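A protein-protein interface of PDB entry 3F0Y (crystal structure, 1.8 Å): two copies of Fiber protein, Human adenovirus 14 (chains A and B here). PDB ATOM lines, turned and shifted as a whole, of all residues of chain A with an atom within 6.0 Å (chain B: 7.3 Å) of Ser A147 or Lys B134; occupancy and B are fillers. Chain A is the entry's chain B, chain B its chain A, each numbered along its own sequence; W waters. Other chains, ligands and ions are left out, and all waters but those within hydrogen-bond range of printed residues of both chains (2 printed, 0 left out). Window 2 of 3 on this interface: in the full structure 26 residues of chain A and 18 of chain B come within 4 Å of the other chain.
NZ of Lys B134 lies within hydrogen-bond range of OH of Tyr A144. The backbone carbonyl oxygen (O) of Thr A145 lies within hydrogen-bond range of the side-chain amino group (NZ) of Lys B134 (2.5 Å). The side-chain amino group (NZ) of Lys B134 is in hydrogen-bond range of the side-chain hydroxyl (OG1) of Thr A192, 2.9 Å away. The side-chain hydroxyl (OH) of Tyr B139 is in hydrogen-bond range of the side-chain hydroxyl (OG1) of Thr A145, 2.7 Å away.
The backbone carbonyl oxygen of Glu B133 sits close to the side-chain amide oxygen of Asn B136, at 3.3 Å. OH of Tyr A144 sits at hydrogen-bond distance from OE2 of Glu A186, at 2.7 Å. The side-chain carboxylate (OE1) of Glu A186 lies within hydrogen-bond range of the side-chain hydroxyl (OG) of Ser A147 (2.6 Å).
Ala A146 touches Lys B134. Ser A147 touches Lys B134 (N to NZ, 3.7 Å). OE2 of Glu B133 touches CE1 of His A149, at 3.8 Å. Thr A193 touches Lys B134. Lys B134 touches Val A195 (CB to CB, 3.8 Å).
Printed residues of chain B within 4 Å of Ser A147: Lys B134 (3.7 Å). Of the printed residues of chain B, Thr A192 touches Lys B134. Of the printed residues of chain B, Thr A193 touches Lys B134 (3.3 Å). Of chain A, only Tyr A144 (3.2 Å), Thr A145 (2.5 Å), Ala A146 (3.6 Å), Ser A147 (3.7 Å), Thr A192 (2.9 Å), Thr A193 (3.3 Å) and Val A195 (3.8 Å) come within 4 Å of Lys B134. The nearest residue of chain A that does not touch Lys B134 is Glu A186 (4.4 Å). The nearest printed residue of chain B that does not touch Thr A145 is Tyr B137 (4.1 Å).
Of the 15 printed residues of chain A, 8 touch a printed residue of chain B. Hydrophobic or aromatic side chains of chain A within 4 Å of the printed part of chain B: Tyr A144, His A149 and Val A195. Hydrophobic or aromatic side chains of chain B that line the printed part of chain A: Tyr B139.
No position is printed for both chains. Of the 9 pairs that touch across the chains among the printed residues, none has its exchanged pair printed and touching as well.
Water W1 lies within hydrogen-bond range of the backbone carbonyl oxygen of Ser B131 (2.6 Å) and the side-chain hydroxyl of Thr A193 (2.7 Å). Water W2 bridges the side-chain hydroxyl of Tyr B139 and the backbone carbonyl oxygen of His A149.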
ATOM      1  N   TYR A 144     -30.993 -13.621   5.729  1.00  0.00           N
ATOM      2  CA  TYR A 144     -30.507 -12.844   4.611  1.00  0.00           C
ATOM      3  C   TYR A 144     -29.370 -13.639   3.974  1.00  0.00           C
ATOM      4  O   TYR A 144     -28.436 -14.056   4.664  1.00  0.00           O
ATOM      5  CB  TYR A 144     -30.013 -11.471   5.080  1.00  0.00           C
ATOM      6  CG  TYR A 144     -29.129 -10.776   4.076  1.00  0.00           C
ATOM      7  CD1 TYR A 144     -29.662 -10.217   2.922  1.00  0.00           C
ATOM      8  CD2 TYR A 144     -27.754 -10.686   4.276  1.00  0.00           C
ATOM      9  CE1 TYR A 144     -28.854  -9.584   1.994  1.00  0.00           C
ATOM     10  CE2 TYR A 144     -26.940 -10.054   3.355  1.00  0.00           C
ATOM     11  CZ  TYR A 144     -27.495  -9.508   2.215  1.00  0.00           C
ATOM     12  OH  TYR A 144     -26.689  -8.882   1.296  1.00  0.00           O
ATOM     13  N   THR A 145     -29.463 -13.873   2.670  1.00  0.00           N
ATOM     14  CA  THR A 145     -28.387 -14.525   1.933  1.00  0.00           C
ATOM     15  C   THR A 145     -27.390 -13.454   1.505  1.00  0.00           C
ATOM     16  O   THR A 145     -27.716 -12.592   0.693  1.00  0.00           O
ATOM     17  CB  THR A 145     -28.913 -15.271   0.695  1.00  0.00           C
ATOM     18  OG1 THR A 145     -29.887 -16.241   1.103  1.00  0.00           O
ATOM     19  CG2 THR A 145     -27.773 -15.975  -0.038  1.00  0.00           C
ATOM     20  N   ALA A 146     -26.187 -13.506   2.065  1.00  0.00           N
ATOM     21  CA  ALA A 146     -25.163 -12.502   1.780  1.00  0.00           C
ATOM     22  C   ALA A 146     -24.583 -12.699   0.388  1.00  0.00           C
ATOM     23  O   ALA A 146     -24.805 -13.734  -0.251  1.00  0.00           O
ATOM     24  CB  ALA A 146     -24.059 -12.552   2.829  1.00  0.00           C
ATOM     25  N   SER A 147     -23.836 -11.701  -0.076  1.00  0.00           N
ATOM     26  CA  SER A 147     -23.216 -11.745  -1.401  1.00  0.00           C
ATOM     27  C   SER A 147     -22.258 -12.931  -1.579  1.00  0.00           C
ATOM     28  O   SER A 147     -22.039 -13.381  -2.704  1.00  0.00           O
ATOM     29  CB  SER A 147     -22.483 -10.434  -1.684  1.00  0.00           C
ATOM     30  OG  SER A 147     -21.547 -10.155  -0.662  1.00  0.00           O
ATOM     31  N   ASP A 148     -21.692 -13.431  -0.478  1.00  0.00           N
ATOM     32  CA  ASP A 148     -20.882 -14.659  -0.508  1.00  0.00           C
ATOM     33  C   ASP A 148     -21.715 -15.936  -0.324  1.00  0.00           C
ATOM     34  O   ASP A 148     -21.156 -17.025  -0.177  1.00  0.00           O
ATOM     35  CB  ASP A 148     -19.753 -14.609   0.537  1.00  0.00           C
ATOM     36  CG  ASP A 148     -20.263 -14.502   1.969  1.00  0.00           C
ATOM     37  OD1 ASP A 148     -21.492 -14.404   2.175  1.00  0.00           O
ATOM     38  OD2 ASP A 148     -19.421 -14.512   2.893  1.00  0.00           O
ATOM     39  N   HIS A 149     -23.041 -15.786  -0.329  1.00  0.00           N
ATOM     40  CA  HIS A 149     -23.999 -16.898  -0.243  1.00  0.00           C
ATOM     41  C   HIS A 149     -24.060 -17.579   1.130  1.00  0.00           C
ATOM     42  O   HIS A 149     -24.610 -18.675   1.254  1.00  0.00           O
ATOM     43  CB  HIS A 149     -23.754 -17.930  -1.357  1.00  0.00           C
ATOM     44  CG  HIS A 149     -23.641 -17.322  -2.721  1.00  0.00           C
ATOM     45  ND1 HIS A 149     -24.740 -17.062  -3.513  1.00  0.00           N
ATOM     46  CD2 HIS A 149     -22.562 -16.910  -3.427  1.00  0.00           C
ATOM     47  CE1 HIS A 149     -24.339 -16.522  -4.651  1.00  0.00           C
ATOM     48  NE2 HIS A 149     -23.023 -16.418  -4.624  1.00  0.00           N
ATOM     49  N   THR A 150     -23.519 -16.926   2.157  1.00  0.00           N
ATOM     50  CA  THR A 150     -23.700 -17.378   3.533  1.00  0.00           C
ATOM     51  C   THR A 150     -25.037 -16.846   4.052  1.00  0.00           C
ATOM     52  O   THR A 150     -25.487 -15.776   3.637  1.00  0.00           O
ATOM     53  CB  THR A 150     -22.557 -16.904   4.453  1.00  0.00           C
ATOM     54  OG1 THR A 150     -22.513 -15.473   4.481  1.00  0.00           O
ATOM     55  CG2 THR A 150     -21.213 -17.445   3.964  1.00  0.00           C
ATOM     56  N   GLU A 186     -24.459  -7.888   5.676  1.00  0.00           N
ATOM     57  CA  GLU A 186     -23.652  -7.802   4.470  1.00  0.00           C
ATOM     58  C   GLU A 186     -22.381  -7.009   4.745  1.00  0.00           C
ATOM     59  O   GLU A 186     -22.428  -5.795   4.946  1.00  0.00           O
ATOM     60  CB  GLU A 186     -24.450  -7.143   3.344  1.00  0.00           C
ATOM     61  CG  GLU A 186     -23.696  -7.057   2.030  1.00  0.00           C
ATOM     62  CD  GLU A 186     -23.204  -8.404   1.552  1.00  0.00           C
ATOM     63  OE1 GLU A 186     -21.981  -8.550   1.345  1.00  0.00           O
ATOM     64  OE2 GLU A 186     -24.034  -9.325   1.399  1.00  0.00           O
ATOM     65  N   GLY A 187     -21.245  -7.701   4.743  1.00  0.00           N
ATOM     66  CA  GLY A 187     -19.957  -7.080   5.045  1.00  0.00           C
ATOM     67  C   GLY A 187     -19.003  -7.003   3.867  1.00  0.00           C
ATOM     68  O   GLY A 187     -17.866  -6.561   4.025  1.00  0.00           O
ATOM     69  N   GLN A 188     -19.453  -7.425   2.686  1.00  0.00           N
ATOM     70  CA  GLN A 188     -18.567  -7.521   1.521  1.00  0.00           C
ATOM     71  C   GLN A 188     -18.865  -6.523   0.402  1.00  0.00           C
ATOM     72  O   GLN A 188     -18.004  -6.280  -0.448  1.00  0.00           O
ATOM     73  CB  GLN A 188     -18.598  -8.940   0.960  1.00  0.00           C
ATOM     74  CG  GLN A 188     -18.090  -9.993   1.930  1.00  0.00           C
ATOM     75  CD  GLN A 188     -18.040 -11.380   1.316  1.00  0.00           C
ATOM     76  OE1 GLN A 188     -18.268 -11.554   0.116  1.00  0.00           O
ATOM     77  NE2 GLN A 188     -17.743 -12.380   2.139  1.00  0.00           N
ATOM     78  N   THR A 189     -20.063  -5.948   0.387  1.00  0.00           N
ATOM     79  CA  THR A 189     -20.424  -5.010  -0.673  1.00  0.00           C
ATOM     80  C   THR A 189     -21.592  -4.101  -0.304  1.00  0.00           C
ATOM     81  O   THR A 189     -22.425  -4.441   0.535  1.00  0.00           O
ATOM     82  CB  THR A 189     -20.764  -5.756  -1.984  1.00  0.00           C
ATOM     83  OG1 THR A 189     -21.079  -4.807  -3.010  1.00  0.00           O
ATOM     84  CG2 THR A 189     -21.944  -6.705  -1.781  1.00  0.00           C
ATOM     85  N   THR A 192     -25.899  -5.040  -3.152  1.00  0.00           N
ATOM     86  CA  THR A 192     -26.540  -6.347  -3.145  1.00  0.00           C
ATOM     87  C   THR A 192     -27.967  -6.193  -2.624  1.00  0.00           C
ATOM     88  O   THR A 192     -28.239  -5.330  -1.792  1.00  0.00           O
ATOM     89  CB  THR A 192     -25.736  -7.361  -2.300  1.00  0.00           C
ATOM     90  OG1 THR A 192     -26.163  -8.696  -2.601  1.00  0.00           O
ATOM     91  CG2 THR A 192     -25.906  -7.087  -0.823  1.00  0.00           C
ATOM     92  N   THR A 193     -28.874  -7.020  -3.131  1.00  0.00           N
ATOM     93  CA  THR A 193     -30.293  -6.877  -2.818  1.00  0.00           C
ATOM     94  C   THR A 193     -30.611  -7.441  -1.438  1.00  0.00           C
ATOM     95  O   THR A 193     -30.165  -8.532  -1.089  1.00  0.00           O
ATOM     96  CB  THR A 193     -31.160  -7.577  -3.875  1.00  0.00           C
ATOM     97  OG1 THR A 193     -30.840  -7.049  -5.168  1.00  0.00           O
ATOM     98  CG2 THR A 193     -32.645  -7.361  -3.594  1.00  0.00           C
ATOM     99  N   LEU A 194     -31.369  -6.679  -0.655  1.00  0.00           N
ATOM    100  CA  LEU A 194     -31.848  -7.145   0.636  1.00  0.00           C
ATOM    101  C   LEU A 194     -32.998  -8.103   0.378  1.00  0.00           C
ATOM    102  O   LEU A 194     -34.117  -7.681   0.088  1.00  0.00           O
ATOM    103  CB  LEU A 194     -32.295  -5.974   1.516  1.00  0.00           C
ATOM    104  CG  LEU A 194     -32.589  -6.287   2.987  1.00  0.00           C
ATOM    105  CD1 LEU A 194     -32.663  -4.997   3.795  1.00  0.00           C
ATOM    106  CD2 LEU A 194     -33.868  -7.092   3.151  1.00  0.00           C
ATOM    107  N   VAL A 195     -32.701  -9.394   0.446  1.00  0.00           N
ATOM    108  CA  VAL A 195     -33.709 -10.433   0.309  1.00  0.00           C
ATOM    109  C   VAL A 195     -33.780 -11.194   1.622  1.00  0.00           C
ATOM    110  O   VAL A 195     -32.765 -11.660   2.131  1.00  0.00           O
ATOM    111  CB  VAL A 195     -33.371 -11.401  -0.844  1.00  0.00           C
ATOM    112  CG1 VAL A 195     -34.340 -12.580  -0.865  1.00  0.00           C
ATOM    113  CG2 VAL A 195     -33.404 -10.665  -2.172  1.00  0.00           C
ATOM    114  N   TYR B 125     -39.092 -18.703  -8.207  1.00  0.00           N
ATOM    115  CA  TYR B 125     -37.748 -19.268  -8.078  1.00  0.00           C
ATOM    116  C   TYR B 125     -37.168 -19.503  -9.475  1.00  0.00           C
ATOM    117  O   TYR B 125     -37.291 -20.596 -10.036  1.00  0.00           O
ATOM    118  CB  TYR B 125     -37.810 -20.565  -7.262  1.00  0.00           C
ATOM    119  CG  TYR B 125     -38.716 -20.426  -6.062  1.00  0.00           C
ATOM    120  CD1 TYR B 125     -39.964 -21.041  -6.030  1.00  0.00           C
ATOM    121  CD2 TYR B 125     -38.348 -19.633  -4.983  1.00  0.00           C
ATOM    122  CE1 TYR B 125     -40.807 -20.892  -4.945  1.00  0.00           C
ATOM    123  CE2 TYR B 125     -39.183 -19.479  -3.891  1.00  0.00           C
ATOM    124  CZ  TYR B 125     -40.414 -20.110  -3.878  1.00  0.00           C
ATOM    125  OH  TYR B 125     -41.256 -19.964  -2.802  1.00  0.00           O
ATOM    126  N   ASN B 129     -30.813 -16.647 -13.077  1.00  0.00           N
ATOM    127  CA  ASN B 129     -31.058 -15.229 -12.855  1.00  0.00           C
ATOM    128  C   ASN B 129     -30.218 -14.764 -11.671  1.00  0.00           C
ATOM    129  O   ASN B 129     -30.615 -14.922 -10.516  1.00  0.00           O
ATOM    130  CB  ASN B 129     -32.548 -14.975 -12.607  1.00  0.00           C
ATOM    131  CG  ASN B 129     -32.922 -13.504 -12.710  1.00  0.00           C
ATOM    132  OD1 ASN B 129     -32.124 -12.620 -12.399  1.00  0.00           O
ATOM    133  ND2 ASN B 129     -34.147 -13.238 -13.146  1.00  0.00           N
ATOM    134  N   ASN B 130     -29.051 -14.200 -11.973  1.00  0.00           N
ATOM    135  CA  ASN B 130     -28.118 -13.740 -10.945  1.00  0.00           C
ATOM    136  C   ASN B 130     -28.709 -12.657 -10.041  1.00  0.00           C
ATOM    137  O   ASN B 130     -28.448 -12.642  -8.839  1.00  0.00           O
ATOM    138  CB  ASN B 130     -26.823 -13.223 -11.589  1.00  0.00           C
ATOM    139  CG  ASN B 130     -26.002 -14.330 -12.238  1.00  0.00           C
ATOM    140  OD1 ASN B 130     -26.228 -15.519 -12.004  1.00  0.00           O
ATOM    141  ND2 ASN B 130     -25.031 -13.936 -13.054  1.00  0.00           N
ATOM    142  N   SER B 131     -29.510 -11.765 -10.619  1.00  0.00           N
ATOM    143  CA  SER B 131     -30.102 -10.659  -9.861  1.00  0.00           C
ATOM    144  C   SER B 131     -31.127 -11.132  -8.828  1.00  0.00           C
ATOM    145  O   SER B 131     -31.342 -10.460  -7.820  1.00  0.00           O
ATOM    146  CB  SER B 131     -30.742  -9.636 -10.804  1.00  0.00           C
ATOM    147  OG  SER B 131     -31.926 -10.142 -11.391  1.00  0.00           O
ATOM    148  N   ARG B 132     -31.750 -12.283  -9.076  1.00  0.00           N
ATOM    149  CA  ARG B 132     -32.765 -12.834  -8.174  1.00  0.00           C
ATOM    150  C   ARG B 132     -32.325 -14.133  -7.496  1.00  0.00           C
ATOM    151  O   ARG B 132     -33.144 -14.832  -6.898  1.00  0.00           O
ATOM    152  CB  ARG B 132     -34.057 -13.084  -8.947  1.00  0.00           C
ATOM    153  CG  ARG B 132     -34.633 -11.851  -9.622  1.00  0.00           C
ATOM    154  CD  ARG B 132     -35.934 -12.190 -10.315  1.00  0.00           C
ATOM    155  NE  ARG B 132     -36.894 -12.766  -9.376  1.00  0.00           N
ATOM    156  CZ  ARG B 132     -37.944 -13.511  -9.713  1.00  0.00           C
ATOM    157  NH1 ARG B 132     -38.204 -13.790 -10.987  1.00  0.00           N
ATOM    158  NH2 ARG B 132     -38.741 -13.980  -8.759  1.00  0.00           N
ATOM    159  N   GLU B 133     -31.034 -14.443  -7.577  1.00  0.00           N
ATOM    160  CA  GLU B 133     -30.489 -15.702  -7.060  1.00  0.00           C
ATOM    161  C   GLU B 133     -30.794 -15.962  -5.578  1.00  0.00           C
ATOM    162  O   GLU B 133     -30.979 -17.112  -5.180  1.00  0.00           O
ATOM    163  CB  GLU B 133     -28.978 -15.742  -7.299  1.00  0.00           C
ATOM    164  CG  GLU B 133     -28.288 -17.006  -6.810  1.00  0.00           C
ATOM    165  CD  GLU B 133     -26.888 -17.169  -7.371  1.00  0.00           C
ATOM    166  OE1 GLU B 133     -26.322 -16.175  -7.881  1.00  0.00           O
ATOM    167  OE2 GLU B 133     -26.353 -18.297  -7.298  1.00  0.00           O
ATOM    168  N   LYS B 134     -30.845 -14.901  -4.773  1.00  0.00           N
ATOM    169  CA  LYS B 134     -31.104 -15.027  -3.334  1.00  0.00           C
ATOM    170  C   LYS B 134     -32.501 -15.568  -3.030  1.00  0.00           C
ATOM    171  O   LYS B 134     -32.713 -16.196  -1.995  1.00  0.00           O
ATOM    172  CB  LYS B 134     -30.939 -13.678  -2.625  1.00  0.00           C
ATOM    173  CG  LYS B 134     -29.533 -13.097  -2.654  1.00  0.00           C
ATOM    174  CD  LYS B 134     -29.524 -11.706  -2.031  1.00  0.00           C
ATOM    175  CE  LYS B 134     -28.238 -10.944  -2.307  1.00  0.00           C
ATOM    176  NZ  LYS B 134     -27.314 -10.917  -1.146  1.00  0.00           N
ATOM    177  N   GLU B 135     -33.447 -15.318  -3.932  1.00  0.00           N
ATOM    178  CA  GLU B 135     -34.840 -15.724  -3.733  1.00  0.00           C
ATOM    179  C   GLU B 135     -35.041 -17.239  -3.834  1.00  0.00           C
ATOM    180  O   GLU B 135     -36.065 -17.761  -3.394  1.00  0.00           O
ATOM    181  CB  GLU B 135     -35.745 -15.003  -4.737  1.00  0.00           C
ATOM    182  CG  GLU B 135     -35.742 -13.487  -4.572  1.00  0.00           C
ATOM    183  CD  GLU B 135     -36.485 -12.773  -5.681  1.00  0.00           C
ATOM    184  OE1 GLU B 135     -37.633 -13.160  -5.971  1.00  0.00           O
ATOM    185  OE2 GLU B 135     -35.927 -11.814  -6.252  1.00  0.00           O
ATOM    186  N   ASN B 136     -34.058 -17.936  -4.399  1.00  0.00           N
ATOM    187  CA  ASN B 136     -34.115 -19.388  -4.558  1.00  0.00           C
ATOM    188  C   ASN B 136     -33.818 -20.174  -3.279  1.00  0.00           C
ATOM    189  O   ASN B 136     -33.977 -21.394  -3.261  1.00  0.00           O
ATOM    190  CB  ASN B 136     -33.141 -19.827  -5.657  1.00  0.00           C
ATOM    191  CG  ASN B 136     -33.523 -19.293  -7.020  1.00  0.00           C
ATOM    192  OD1 ASN B 136     -33.031 -18.253  -7.453  1.00  0.00           O
ATOM    193  ND2 ASN B 136     -34.419 -19.995  -7.701  1.00  0.00           N
ATOM    194  N   TYR B 137     -33.404 -19.484  -2.216  1.00  0.00           N
ATOM    195  CA  TYR B 137     -32.929 -20.144  -1.002  1.00  0.00           C
ATOM    196  C   TYR B 137     -33.928 -20.115   0.154  1.00  0.00           C
ATOM    197  O   TYR B 137     -34.539 -19.086   0.450  1.00  0.00           O
ATOM    198  CB  TYR B 137     -31.610 -19.521  -0.544  1.00  0.00           C
ATOM    199  CG  TYR B 137     -30.473 -19.731  -1.513  1.00  0.00           C
ATOM    200  CD1 TYR B 137     -30.128 -18.746  -2.434  1.00  0.00           C
ATOM    201  CD2 TYR B 137     -29.736 -20.913  -1.509  1.00  0.00           C
ATOM    202  CE1 TYR B 137     -29.079 -18.931  -3.326  1.00  0.00           C
ATOM    203  CE2 TYR B 137     -28.684 -21.107  -2.400  1.00  0.00           C
ATOM    204  CZ  TYR B 137     -28.362 -20.111  -3.305  1.00  0.00           C
ATOM    205  OH  TYR B 137     -27.324 -20.290  -4.194  1.00  0.00           O
ATOM    206  N   ILE B 138     -34.073 -21.269   0.798  1.00  0.00           N
ATOM    207  CA  ILE B 138     -34.867 -21.423   2.009  1.00  0.00           C
ATOM    208  C   ILE B 138     -33.970 -22.071   3.058  1.00  0.00           C
ATOM    209  O   ILE B 138     -33.188 -22.969   2.739  1.00  0.00           O
ATOM    210  CB  ILE B 138     -36.103 -22.309   1.751  1.00  0.00           C
ATOM    211  CG1 ILE B 138     -37.139 -21.553   0.918  1.00  0.00           C
ATOM    212  CG2 ILE B 138     -36.725 -22.776   3.060  1.00  0.00           C
ATOM    213  CD1 ILE B 138     -38.222 -22.441   0.346  1.00  0.00           C
ATOM    214  N   TYR B 139     -34.070 -21.610   4.302  1.00  0.00           N
ATOM    215  CA  TYR B 139     -33.215 -22.107   5.374  1.00  0.00           C
ATOM    216  C   TYR B 139     -34.024 -22.549   6.583  1.00  0.00           C
ATOM    217  O   TYR B 139     -35.130 -22.063   6.824  1.00  0.00           O
ATOM    218  CB  TYR B 139     -32.226 -21.032   5.814  1.00  0.00           C
ATOM    219  CG  TYR B 139     -31.415 -20.440   4.686  1.00  0.00           C
ATOM    220  CD1 TYR B 139     -31.809 -19.260   4.071  1.00  0.00           C
ATOM    221  CD2 TYR B 139     -30.251 -21.059   4.238  1.00  0.00           C
ATOM    222  CE1 TYR B 139     -31.069 -18.704   3.037  1.00  0.00           C
ATOM    223  CE2 TYR B 139     -29.503 -20.513   3.202  1.00  0.00           C
ATOM    224  CZ  TYR B 139     -29.916 -19.334   2.610  1.00  0.00           C
ATOM    225  OH  TYR B 139     -29.181 -18.785   1.585  1.00  0.00           O
ATOM    226  N   GLN B 162     -33.086 -22.424  -9.701  1.00  0.00           N
ATOM    227  CA  GLN B 162     -31.789 -21.736  -9.818  1.00  0.00           C
ATOM    228  C   GLN B 162     -30.918 -22.238 -10.971  1.00  0.00           C
ATOM    229  O   GLN B 162     -30.567 -21.465 -11.865  1.00  0.00           O
ATOM    230  CB  GLN B 162     -31.003 -21.778  -8.494  1.00  0.00           C
ATOM    231  CG  GLN B 162     -29.637 -21.093  -8.544  1.00  0.00           C
ATOM    232  CD  GLN B 162     -29.694 -19.701  -9.138  1.00  0.00           C
ATOM    233  OE1 GLN B 162     -30.496 -18.870  -8.715  1.00  0.00           O
ATOM    234  NE2 GLN B 162     -28.843 -19.438 -10.124  1.00  0.00           N
HETATM  235  O   HOH W   1     -30.211  -8.106  -7.565  1.00  0.00           O
HETATM  236  O   HOH W   2     -26.910 -20.006   0.964  1.00  0.00           O
